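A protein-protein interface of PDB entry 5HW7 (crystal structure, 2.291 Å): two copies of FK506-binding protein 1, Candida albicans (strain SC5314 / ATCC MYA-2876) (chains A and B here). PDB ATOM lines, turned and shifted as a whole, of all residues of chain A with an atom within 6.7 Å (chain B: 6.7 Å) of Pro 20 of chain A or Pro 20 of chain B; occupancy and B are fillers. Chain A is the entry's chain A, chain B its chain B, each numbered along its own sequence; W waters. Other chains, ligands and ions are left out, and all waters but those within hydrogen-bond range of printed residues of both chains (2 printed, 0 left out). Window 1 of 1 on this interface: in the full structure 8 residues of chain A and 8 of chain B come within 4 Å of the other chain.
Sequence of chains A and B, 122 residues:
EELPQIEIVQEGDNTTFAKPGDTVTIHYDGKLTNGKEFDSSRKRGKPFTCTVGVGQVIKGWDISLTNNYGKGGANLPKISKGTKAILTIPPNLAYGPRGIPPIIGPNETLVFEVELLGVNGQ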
ATOM      1  N   ALA A  18      27.961  24.273 -11.379  1.00  0.00           N
ATOM      2  CA  ALA A  18      27.154  23.106 -11.078  1.00  0.00           C
ATOM      3  C   ALA A  18      26.106  22.848 -12.157  1.00  0.00           C
ATOM      4  O   ALA A  18      25.536  23.780 -12.712  1.00  0.00           O
ATOM      5  CB  ALA A  18      26.486  23.259  -9.724  1.00  0.00           C
ATOM      6  N   LYS A  19      25.825  21.571 -12.400  1.00  0.00           N
ATOM      7  CA  LYS A  19      24.825  21.150 -13.360  1.00  0.00           C
ATOM      8  C   LYS A  19      23.834  20.320 -12.573  1.00  0.00           C
ATOM      9  O   LYS A  19      24.116  19.969 -11.428  1.00  0.00           O
ATOM     10  CB  LYS A  19      25.410  20.333 -14.518  1.00  0.00           C
ATOM     11  CG  LYS A  19      26.503  20.985 -15.337  1.00  0.00           C
ATOM     12  CD  LYS A  19      26.899  20.031 -16.471  1.00  0.00           C
ATOM     13  CE  LYS A  19      28.168  20.457 -17.197  1.00  0.00           C
ATOM     14  NZ  LYS A  19      28.095  20.109 -18.656  1.00  0.00           N
ATOM     15  N   PRO A  20      22.646  20.050 -13.149  1.00  0.00           N
ATOM     16  CA  PRO A  20      21.664  19.273 -12.393  1.00  0.00           C
ATOM     17  C   PRO A  20      22.186  17.889 -12.024  1.00  0.00           C
ATOM     18  O   PRO A  20      22.779  17.221 -12.861  1.00  0.00           O
ATOM     19  CB  PRO A  20      20.483  19.173 -13.361  1.00  0.00           C
ATOM     20  CG  PRO A  20      20.631  20.350 -14.245  1.00  0.00           C
ATOM     21  CD  PRO A  20      22.103  20.472 -14.454  1.00  0.00           C
ATOM     22  N   GLY A  21      21.993  17.491 -10.772  1.00  0.00           N
ATOM     23  CA  GLY A  21      22.469  16.219 -10.277  1.00  0.00           C
ATOM     24  C   GLY A  21      23.843  16.302  -9.660  1.00  0.00           C
ATOM     25  O   GLY A  21      24.306  15.359  -9.020  1.00  0.00           O
ATOM     26  N   ASP A  22      24.478  17.455  -9.797  1.00  0.00           N
ATOM     27  CA  ASP A  22      25.711  17.708  -9.065  1.00  0.00           C
ATOM     28  C   ASP A  22      25.417  17.994  -7.610  1.00  0.00           C
ATOM     29  O   ASP A  22      24.305  18.374  -7.226  1.00  0.00           O
ATOM     30  CB  ASP A  22      26.493  18.893  -9.644  1.00  0.00           C
ATOM     31  CG  ASP A  22      27.216  18.559 -10.930  1.00  0.00           C
ATOM     32  OD1 ASP A  22      27.341  17.355 -11.265  1.00  0.00           O
ATOM     33  OD2 ASP A  22      27.659  19.521 -11.606  1.00  0.00           O
ATOM     34  N   THR A  51      22.224  18.109  -3.331  1.00  0.00           N
ATOM     35  CA  THR A  51      22.161  17.886  -4.764  1.00  0.00           C
ATOM     36  C   THR A  51      21.272  18.964  -5.350  1.00  0.00           C
ATOM     37  O   THR A  51      20.188  19.216  -4.843  1.00  0.00           O
ATOM     38  CB  THR A  51      21.613  16.482  -5.127  1.00  0.00           C
ATOM     39  OG1 THR A  51      22.386  15.481  -4.455  1.00  0.00           O
ATOM     40  CG2 THR A  51      21.753  16.235  -6.625  1.00  0.00           C
ATOM     41  N   VAL A  52      21.746  19.625  -6.399  1.00  0.00           N
ATOM     42  CA  VAL A  52      20.995  20.713  -7.023  1.00  0.00           C
ATOM     43  C   VAL A  52      20.382  20.299  -8.363  1.00  0.00           C
ATOM     44  O   VAL A  52      20.856  19.363  -9.025  1.00  0.00           O
ATOM     45  CB  VAL A  52      21.870  21.967  -7.258  1.00  0.00           C
ATOM     46  CG1 VAL A  52      22.102  22.733  -5.969  1.00  0.00           C
ATOM     47  CG2 VAL A  52      23.185  21.588  -7.953  1.00  0.00           C
ATOM     48  N   GLY A  53      19.286  20.961  -8.722  1.00  0.00           N
ATOM     49  CA  GLY A  53      18.623  20.691  -9.983  1.00  0.00           C
ATOM     50  C   GLY A  53      17.636  19.547  -9.983  1.00  0.00           C
ATOM     51  O   GLY A  53      17.124  19.176 -11.043  1.00  0.00           O
ATOM     52  N   VAL A  54      17.408  18.941  -8.818  1.00  0.00           N
ATOM     53  CA  VAL A  54      16.513  17.794  -8.741  1.00  0.00           C
ATOM     54  C   VAL A  54      15.312  17.932  -7.806  1.00  0.00           C
ATOM     55  O   VAL A  54      14.681  16.926  -7.491  1.00  0.00           O
ATOM     56  CB  VAL A  54      17.290  16.533  -8.344  1.00  0.00           C
ATOM     57  CG1 VAL A  54      18.463  16.331  -9.290  1.00  0.00           C
ATOM     58  CG2 VAL A  54      17.785  16.641  -6.915  1.00  0.00           C
ATOM     59  N   THR A  66      22.140  26.189 -10.764  1.00  0.00           N
ATOM     60  CA  THR A  66      22.360  25.495 -12.030  1.00  0.00           C
ATOM     61  C   THR A  66      22.180  26.385 -13.233  1.00  0.00           C
ATOM     62  O   THR A  66      22.143  25.882 -14.360  1.00  0.00           O
ATOM     63  CB  THR A  66      21.453  24.266 -12.230  1.00  0.00           C
ATOM     64  OG1 THR A  66      20.096  24.696 -12.438  1.00  0.00           O
ATOM     65  CG2 THR A  66      21.550  23.324 -11.033  1.00  0.00           C
ATOM     66  N   ASN A  68      19.396  27.978 -14.283  1.00  0.00           N
ATOM     67  CA  ASN A  68      18.162  27.499 -14.916  1.00  0.00           C
ATOM     68  C   ASN A  68      18.339  26.162 -15.620  1.00  0.00           C
ATOM     69  O   ASN A  68      17.977  26.013 -16.785  1.00  0.00           O
ATOM     70  CB  ASN A  68      17.616  28.539 -15.905  1.00  0.00           C
ATOM     71  CG  ASN A  68      16.097  28.489 -16.034  1.00  0.00           C
ATOM     72  OD1 ASN A  68      15.405  27.782 -15.282  1.00  0.00           O
ATOM     73  ND2 ASN A  68      15.572  29.231 -16.996  1.00  0.00           N
ATOM     74  N   TYR A  69      18.942  25.212 -14.910  1.00  0.00           N
ATOM     75  CA  TYR A  69      19.123  23.849 -15.385  1.00  0.00           C
ATOM     76  C   TYR A  69      20.005  23.765 -16.630  1.00  0.00           C
ATOM     77  O   TYR A  69      19.869  22.845 -17.426  1.00  0.00           O
ATOM     78  CB  TYR A  69      17.752  23.192 -15.634  1.00  0.00           C
ATOM     79  CG  TYR A  69      16.818  23.325 -14.452  1.00  0.00           C
ATOM     80  CD1 TYR A  69      16.790  22.361 -13.448  1.00  0.00           C
ATOM     81  CD2 TYR A  69      15.941  24.394 -14.351  1.00  0.00           C
ATOM     82  CE1 TYR A  69      15.932  22.482 -12.357  1.00  0.00           C
ATOM     83  CE2 TYR A  69      15.092  24.531 -13.265  1.00  0.00           C
ATOM     84  CZ  TYR A  69      15.083  23.570 -12.275  1.00  0.00           C
ATOM     85  OH  TYR A  69      14.223  23.715 -11.198  1.00  0.00           O
ATOM     86  N   GLY A  70      20.905  24.730 -16.788  1.00  0.00           N
ATOM     87  CA  GLY A  70      21.811  24.774 -17.926  1.00  0.00           C
ATOM     88  C   GLY A  70      21.291  25.537 -19.135  1.00  0.00           C
ATOM     89  O   GLY A  70      22.038  25.803 -20.079  1.00  0.00           O
ATOM     90  N   LYS A  71      19.999  25.851 -19.124  1.00  0.00           N
ATOM     91  CA  LYS A  71      19.371  26.719 -20.128  1.00  0.00           C
ATOM     92  C   LYS A  71      19.720  28.216 -20.054  1.00  0.00           C
ATOM     93  O   LYS A  71      19.627  28.917 -21.049  1.00  0.00           O
ATOM     94  CB  LYS A  71      17.846  26.545 -20.079  1.00  0.00           C
ATOM     95  CG  LYS A  71      17.319  25.118 -20.312  1.00  0.00           C
ATOM     96  CD  LYS A  71      18.278  24.223 -21.105  1.00  0.00           C
ATOM     97  CE  LYS A  71      17.610  23.651 -22.362  1.00  0.00           C
ATOM     98  NZ  LYS A  71      18.383  22.542 -22.989  1.00  0.00           N
ATOM     99  N   ALA B  18      16.584  13.548 -24.024  1.00  0.00           N
ATOM    100  CA  ALA B  18      16.141  14.746 -23.331  1.00  0.00           C
ATOM    101  C   ALA B  18      17.145  15.072 -22.248  1.00  0.00           C
ATOM    102  O   ALA B  18      17.711  14.169 -21.625  1.00  0.00           O
ATOM    103  CB  ALA B  18      14.753  14.562 -22.739  1.00  0.00           C
ATOM    104  N   LYS B  19      17.339  16.363 -22.007  1.00  0.00           N
ATOM    105  CA  LYS B  19      18.273  16.827 -20.997  1.00  0.00           C
ATOM    106  C   LYS B  19      17.437  17.703 -20.074  1.00  0.00           C
ATOM    107  O   LYS B  19      16.353  18.122 -20.469  1.00  0.00           O
ATOM    108  CB  LYS B  19      19.416  17.606 -21.647  1.00  0.00           C
ATOM    109  CG  LYS B  19      20.678  16.790 -21.850  1.00  0.00           C
ATOM    110  CD  LYS B  19      21.708  17.562 -22.651  1.00  0.00           C
ATOM    111  CE  LYS B  19      22.543  16.614 -23.499  1.00  0.00           C
ATOM    112  NZ  LYS B  19      23.651  15.990 -22.727  1.00  0.00           N
ATOM    113  N   PRO B  20      17.898  17.944 -18.835  1.00  0.00           N
ATOM    114  CA  PRO B  20      17.042  18.740 -17.953  1.00  0.00           C
ATOM    115  C   PRO B  20      16.791  20.122 -18.548  1.00  0.00           C
ATOM    116  O   PRO B  20      17.712  20.743 -19.068  1.00  0.00           O
ATOM    117  CB  PRO B  20      17.864  18.826 -16.668  1.00  0.00           C
ATOM    118  CG  PRO B  20      18.640  17.548 -16.653  1.00  0.00           C
ATOM    119  CD  PRO B  20      19.007  17.316 -18.097  1.00  0.00           C
ATOM    120  N   GLY B  21      15.539  20.567 -18.530  1.00  0.00           N
ATOM    121  CA  GLY B  21      15.186  21.842 -19.119  1.00  0.00           C
ATOM    122  C   GLY B  21      14.833  21.735 -20.587  1.00  0.00           C
ATOM    123  O   GLY B  21      14.459  22.723 -21.216  1.00  0.00           O
ATOM    124  N   ASP B  22      14.975  20.540 -21.149  1.00  0.00           N
ATOM    125  CA  ASP B  22      14.478  20.297 -22.493  1.00  0.00           C
ATOM    126  C   ASP B  22      12.969  20.156 -22.494  1.00  0.00           C
ATOM    127  O   ASP B  22      12.351  19.828 -21.479  1.00  0.00           O
ATOM    128  CB  ASP B  22      15.103  19.052 -23.107  1.00  0.00           C
ATOM    129  CG  ASP B  22      16.507  19.292 -23.604  1.00  0.00           C
ATOM    130  OD1 ASP B  22      16.890  20.469 -23.791  1.00  0.00           O
ATOM    131  OD2 ASP B  22      17.227  18.300 -23.814  1.00  0.00           O
ATOM    132  N   THR B  51       8.151  20.435 -19.905  1.00  0.00           N
ATOM    133  CA  THR B  51       9.574  20.615 -19.683  1.00  0.00           C
ATOM    134  C   THR B  51       9.987  19.537 -18.681  1.00  0.00           C
ATOM    135  O   THR B  51       9.308  19.340 -17.666  1.00  0.00           O
ATOM    136  CB  THR B  51       9.899  22.020 -19.146  1.00  0.00           C
ATOM    137  OG1 THR B  51       9.199  22.998 -19.920  1.00  0.00           O
ATOM    138  CG2 THR B  51      11.378  22.293 -19.236  1.00  0.00           C
ATOM    139  N   VAL B  52      11.054  18.799 -18.977  1.00  0.00           N
ATOM    140  CA  VAL B  52      11.465  17.702 -18.096  1.00  0.00           C
ATOM    141  C   VAL B  52      12.675  18.079 -17.275  1.00  0.00           C
ATOM    142  O   VAL B  52      13.447  18.955 -17.654  1.00  0.00           O
ATOM    143  CB  VAL B  52      11.772  16.390 -18.869  1.00  0.00           C
ATOM    144  CG1 VAL B  52      10.486  15.775 -19.366  1.00  0.00           C
ATOM    145  CG2 VAL B  52      12.745  16.637 -20.012  1.00  0.00           C
ATOM    146  N   GLY B  53      12.818  17.432 -16.128  1.00  0.00           N
ATOM    147  CA  GLY B  53      13.970  17.648 -15.269  1.00  0.00           C
ATOM    148  C   GLY B  53      13.849  18.844 -14.348  1.00  0.00           C
ATOM    149  O   GLY B  53      14.750  19.110 -13.561  1.00  0.00           O
ATOM    150  N   VAL B  54      12.742  19.571 -14.438  1.00  0.00           N
ATOM    151  CA  VAL B  54      12.585  20.794 -13.655  1.00  0.00           C
ATOM    152  C   VAL B  54      11.472  20.773 -12.602  1.00  0.00           C
ATOM    153  O   VAL B  54      11.093  21.828 -12.099  1.00  0.00           O
ATOM    154  CB  VAL B  54      12.337  22.006 -14.586  1.00  0.00           C
ATOM    155  CG1 VAL B  54      13.461  22.118 -15.609  1.00  0.00           C
ATOM    156  CG2 VAL B  54      10.980  21.888 -15.283  1.00  0.00           C
ATOM    157  N   THR B  66      14.900  11.998 -18.388  1.00  0.00           N
ATOM    158  CA  THR B  66      16.215  12.666 -18.456  1.00  0.00           C
ATOM    159  C   THR B  66      17.364  11.717 -18.086  1.00  0.00           C
ATOM    160  O   THR B  66      18.511  12.158 -17.953  1.00  0.00           O
ATOM    161  CB  THR B  66      16.312  13.926 -17.555  1.00  0.00           C
ATOM    162  OG1 THR B  66      16.348  13.538 -16.177  1.00  0.00           O
ATOM    163  CG2 THR B  66      15.149  14.876 -17.803  1.00  0.00           C
ATOM    164  N   ASN B  68      17.881  10.155 -15.066  1.00  0.00           N
ATOM    165  CA  ASN B  68      18.376  10.601 -13.762  1.00  0.00           C
ATOM    166  C   ASN B  68      19.230  11.855 -13.856  1.00  0.00           C
ATOM    167  O   ASN B  68      20.365  11.901 -13.360  1.00  0.00           O
ATOM    168  CB  ASN B  68      19.153   9.486 -13.054  1.00  0.00           C
ATOM    169  CG  ASN B  68      19.134   9.649 -11.544  1.00  0.00           C
ATOM    170  OD1 ASN B  68      18.234  10.289 -10.992  1.00  0.00           O
ATOM    171  ND2 ASN B  68      20.100   9.045 -10.867  1.00  0.00           N
ATOM    172  N   TYR B  69      18.678  12.845 -14.558  1.00  0.00           N
ATOM    173  CA  TYR B  69      19.262  14.178 -14.690  1.00  0.00           C
ATOM    174  C   TYR B  69      20.614  14.082 -15.386  1.00  0.00           C
ATOM    175  O   TYR B  69      21.478  14.941 -15.224  1.00  0.00           O
ATOM    176  CB  TYR B  69      19.364  14.853 -13.318  1.00  0.00           C
ATOM    177  CG  TYR B  69      18.046  14.860 -12.574  1.00  0.00           C
ATOM    178  CD1 TYR B  69      17.161  15.927 -12.709  1.00  0.00           C
ATOM    179  CD2 TYR B  69      17.682  13.809 -11.737  1.00  0.00           C
ATOM    180  CE1 TYR B  69      15.944  15.943 -12.042  1.00  0.00           C
ATOM    181  CE2 TYR B  69      16.472  13.820 -11.061  1.00  0.00           C
ATOM    182  CZ  TYR B  69      15.601  14.887 -11.220  1.00  0.00           C
ATOM    183  OH  TYR B  69      14.386  14.913 -10.554  1.00  0.00           O
ATOM    184  N   GLY B  70      20.782  13.008 -16.151  1.00  0.00           N
ATOM    185  CA  GLY B  70      21.970  12.770 -16.948  1.00  0.00           C
ATOM    186  C   GLY B  70      23.045  12.012 -16.201  1.00  0.00           C
ATOM    187  O   GLY B  70      24.035  11.583 -16.788  1.00  0.00           O
ATOM    188  N   LYS B  71      22.859  11.859 -14.898  1.00  0.00           N
ATOM    189  CA  LYS B  71      23.737  11.013 -14.098  1.00  0.00           C
ATOM    190  C   LYS B  71      23.536   9.536 -14.427  1.00  0.00           C
ATOM    191  O   LYS B  71      24.484   8.756 -14.430  1.00  0.00           O
ATOM    192  CB  LYS B  71      23.515  11.270 -12.608  1.00  0.00           C
ATOM    193  CG  LYS B  71      23.698  12.729 -12.176  1.00  0.00           C
ATOM    194  CD  LYS B  71      24.745  13.487 -12.987  1.00  0.00           C
ATOM    195  CE  LYS B  71      25.855  14.006 -12.088  1.00  0.00           C
ATOM    196  NZ  LYS B  71      26.338  15.355 -12.497  1.00  0.00           N
HETATM  197  O   HOH W   1      22.979  16.954 -15.527  1.00  0.00           O
HETATM  198  O   HOH W   2      14.186  19.345 -10.980  1.00  0.00           O
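Water W1 bridges the backbone carbonyl oxygen (O) of Tyr 69 of chain B (2.5 Å) and the backbone carbonyl oxygen (O) of Pro 20 of chain A (2.7 Å). Water W2 lies within hydrogen-bond range of the backbone carbonyl oxygen of Gly 53 of chain B and the backbone carbonyl oxygen of Gly 53 of chain A.
Among the printed residues, pairs that only touch across the chains: Pro 20 of chain A with Pro 20 of chain B (3.98 Å), Pro 20 of chain A with Tyr 69 of chain B (3.5 Å), Gly 21 of chain A with Lys 71 of chain B (3.7 Å), Gly 53 of chain A with Tyr 69 of chain B (3.6 Å), Val 54 of chain A with Tyr 69 of chain B (3.6 Å), Tyr 69 of chain A with Gly 53 of chain B (3.8 Å), Tyr 69 of chain A with Val 54 of chain B (3.6 Å) and Lys 71 of chain A with Gly 21 of chain B (3.5 Å).
The side-chain carboxylate (OD1) of Asp 22 of chain A lies within salt-bridge range of the side-chain amino group (NZ) of Lys 71 of chain B, at 2.6 Å. NZ of Lys 71 of chain A is in salt-bridge range of OD1 of Asp 22 of chain B, at 2.7 Å. O of Gly 53 of chain B lies close to O of Gly 53 of chain A, 3.5 Å away. The backbone carbonyl oxygen (O) of Pro 20 of chain B sits close to the backbone carbonyl oxygen (O) of Tyr 69 of chain A (3.4 Å).
Of the printed residues of chain B, Pro 20 of chain A touches Pro 20 and Tyr 69. Printed residues of chain B within 4 Å of Gly 53 of chain A: Gly 53 (3.5 Å) and Tyr 69 (3.6 Å). Of the printed residues of chain A, Gly 21 of chain B touches Lys 71 (3.5 Å).
N of Gly 21 of chain A sits at hydrogen-bond distance from O of Val 52 of chain A (2.8 Å). The backbone NH (N) of Tyr 69 of chain A is in hydrogen-bond range of the side-chain hydroxyl (OG1) of Thr 66 of chain A, at 2.8 Å. The backbone NH of Lys 19 of chain B sits at hydrogen-bond distance from the side-chain carboxylate of Asp 22 of chain B (2.7 Å). The backbone NH (N) of Gly 21 of chain B sits at hydrogen-bond distance from the backbone carbonyl oxygen (O) of Val 52 of chain B, at 2.8 Å. The backbone carbonyl oxygen (O) of Asp 22 of chain B is in hydrogen-bond range of the backbone NH (N) of Val 52 of chain B (3.0 Å). OG1 of Thr 66 of chain B lies within hydrogen-bond range of N of Tyr 69 of chain B, at 2.9 Å.
Pro 20 of chain B touches its own counterpart, Pro 20 of chain A. Gly 21 of chain A touches Lys 71 of chain B, and with the chains exchanged Lys 71 of chain A touches Gly 21 of chain B. Gly 53 of chain B touches its own counterpart, Gly 53 of chain A. Val 54 of chain A touches Tyr 69 of chain B, and with the chains exchanged Tyr 69 of chain A touches Val 54 of chain B. Positions printed for both chains: 18, 19, 20, 21, 22, 51, 52, 53, 54, 66, 68, 69, 70 and 71. Of the 12 pairs that touch across the chains among the printed residues, 12 have their exchanged pair printed and touching as well.
Of the 14 printed residues of chain B, 7 touch a printed residue of chain A. Hydrophobic or aromatic side chains of chain B within 4 Å of the printed part of chain A: Pro 20, Val 54 and Tyr 69. Hydrophobic or aromatic side chains of chain A within 4 Å of the printed part of chain B: Pro 20, Val 54 and Tyr 69.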
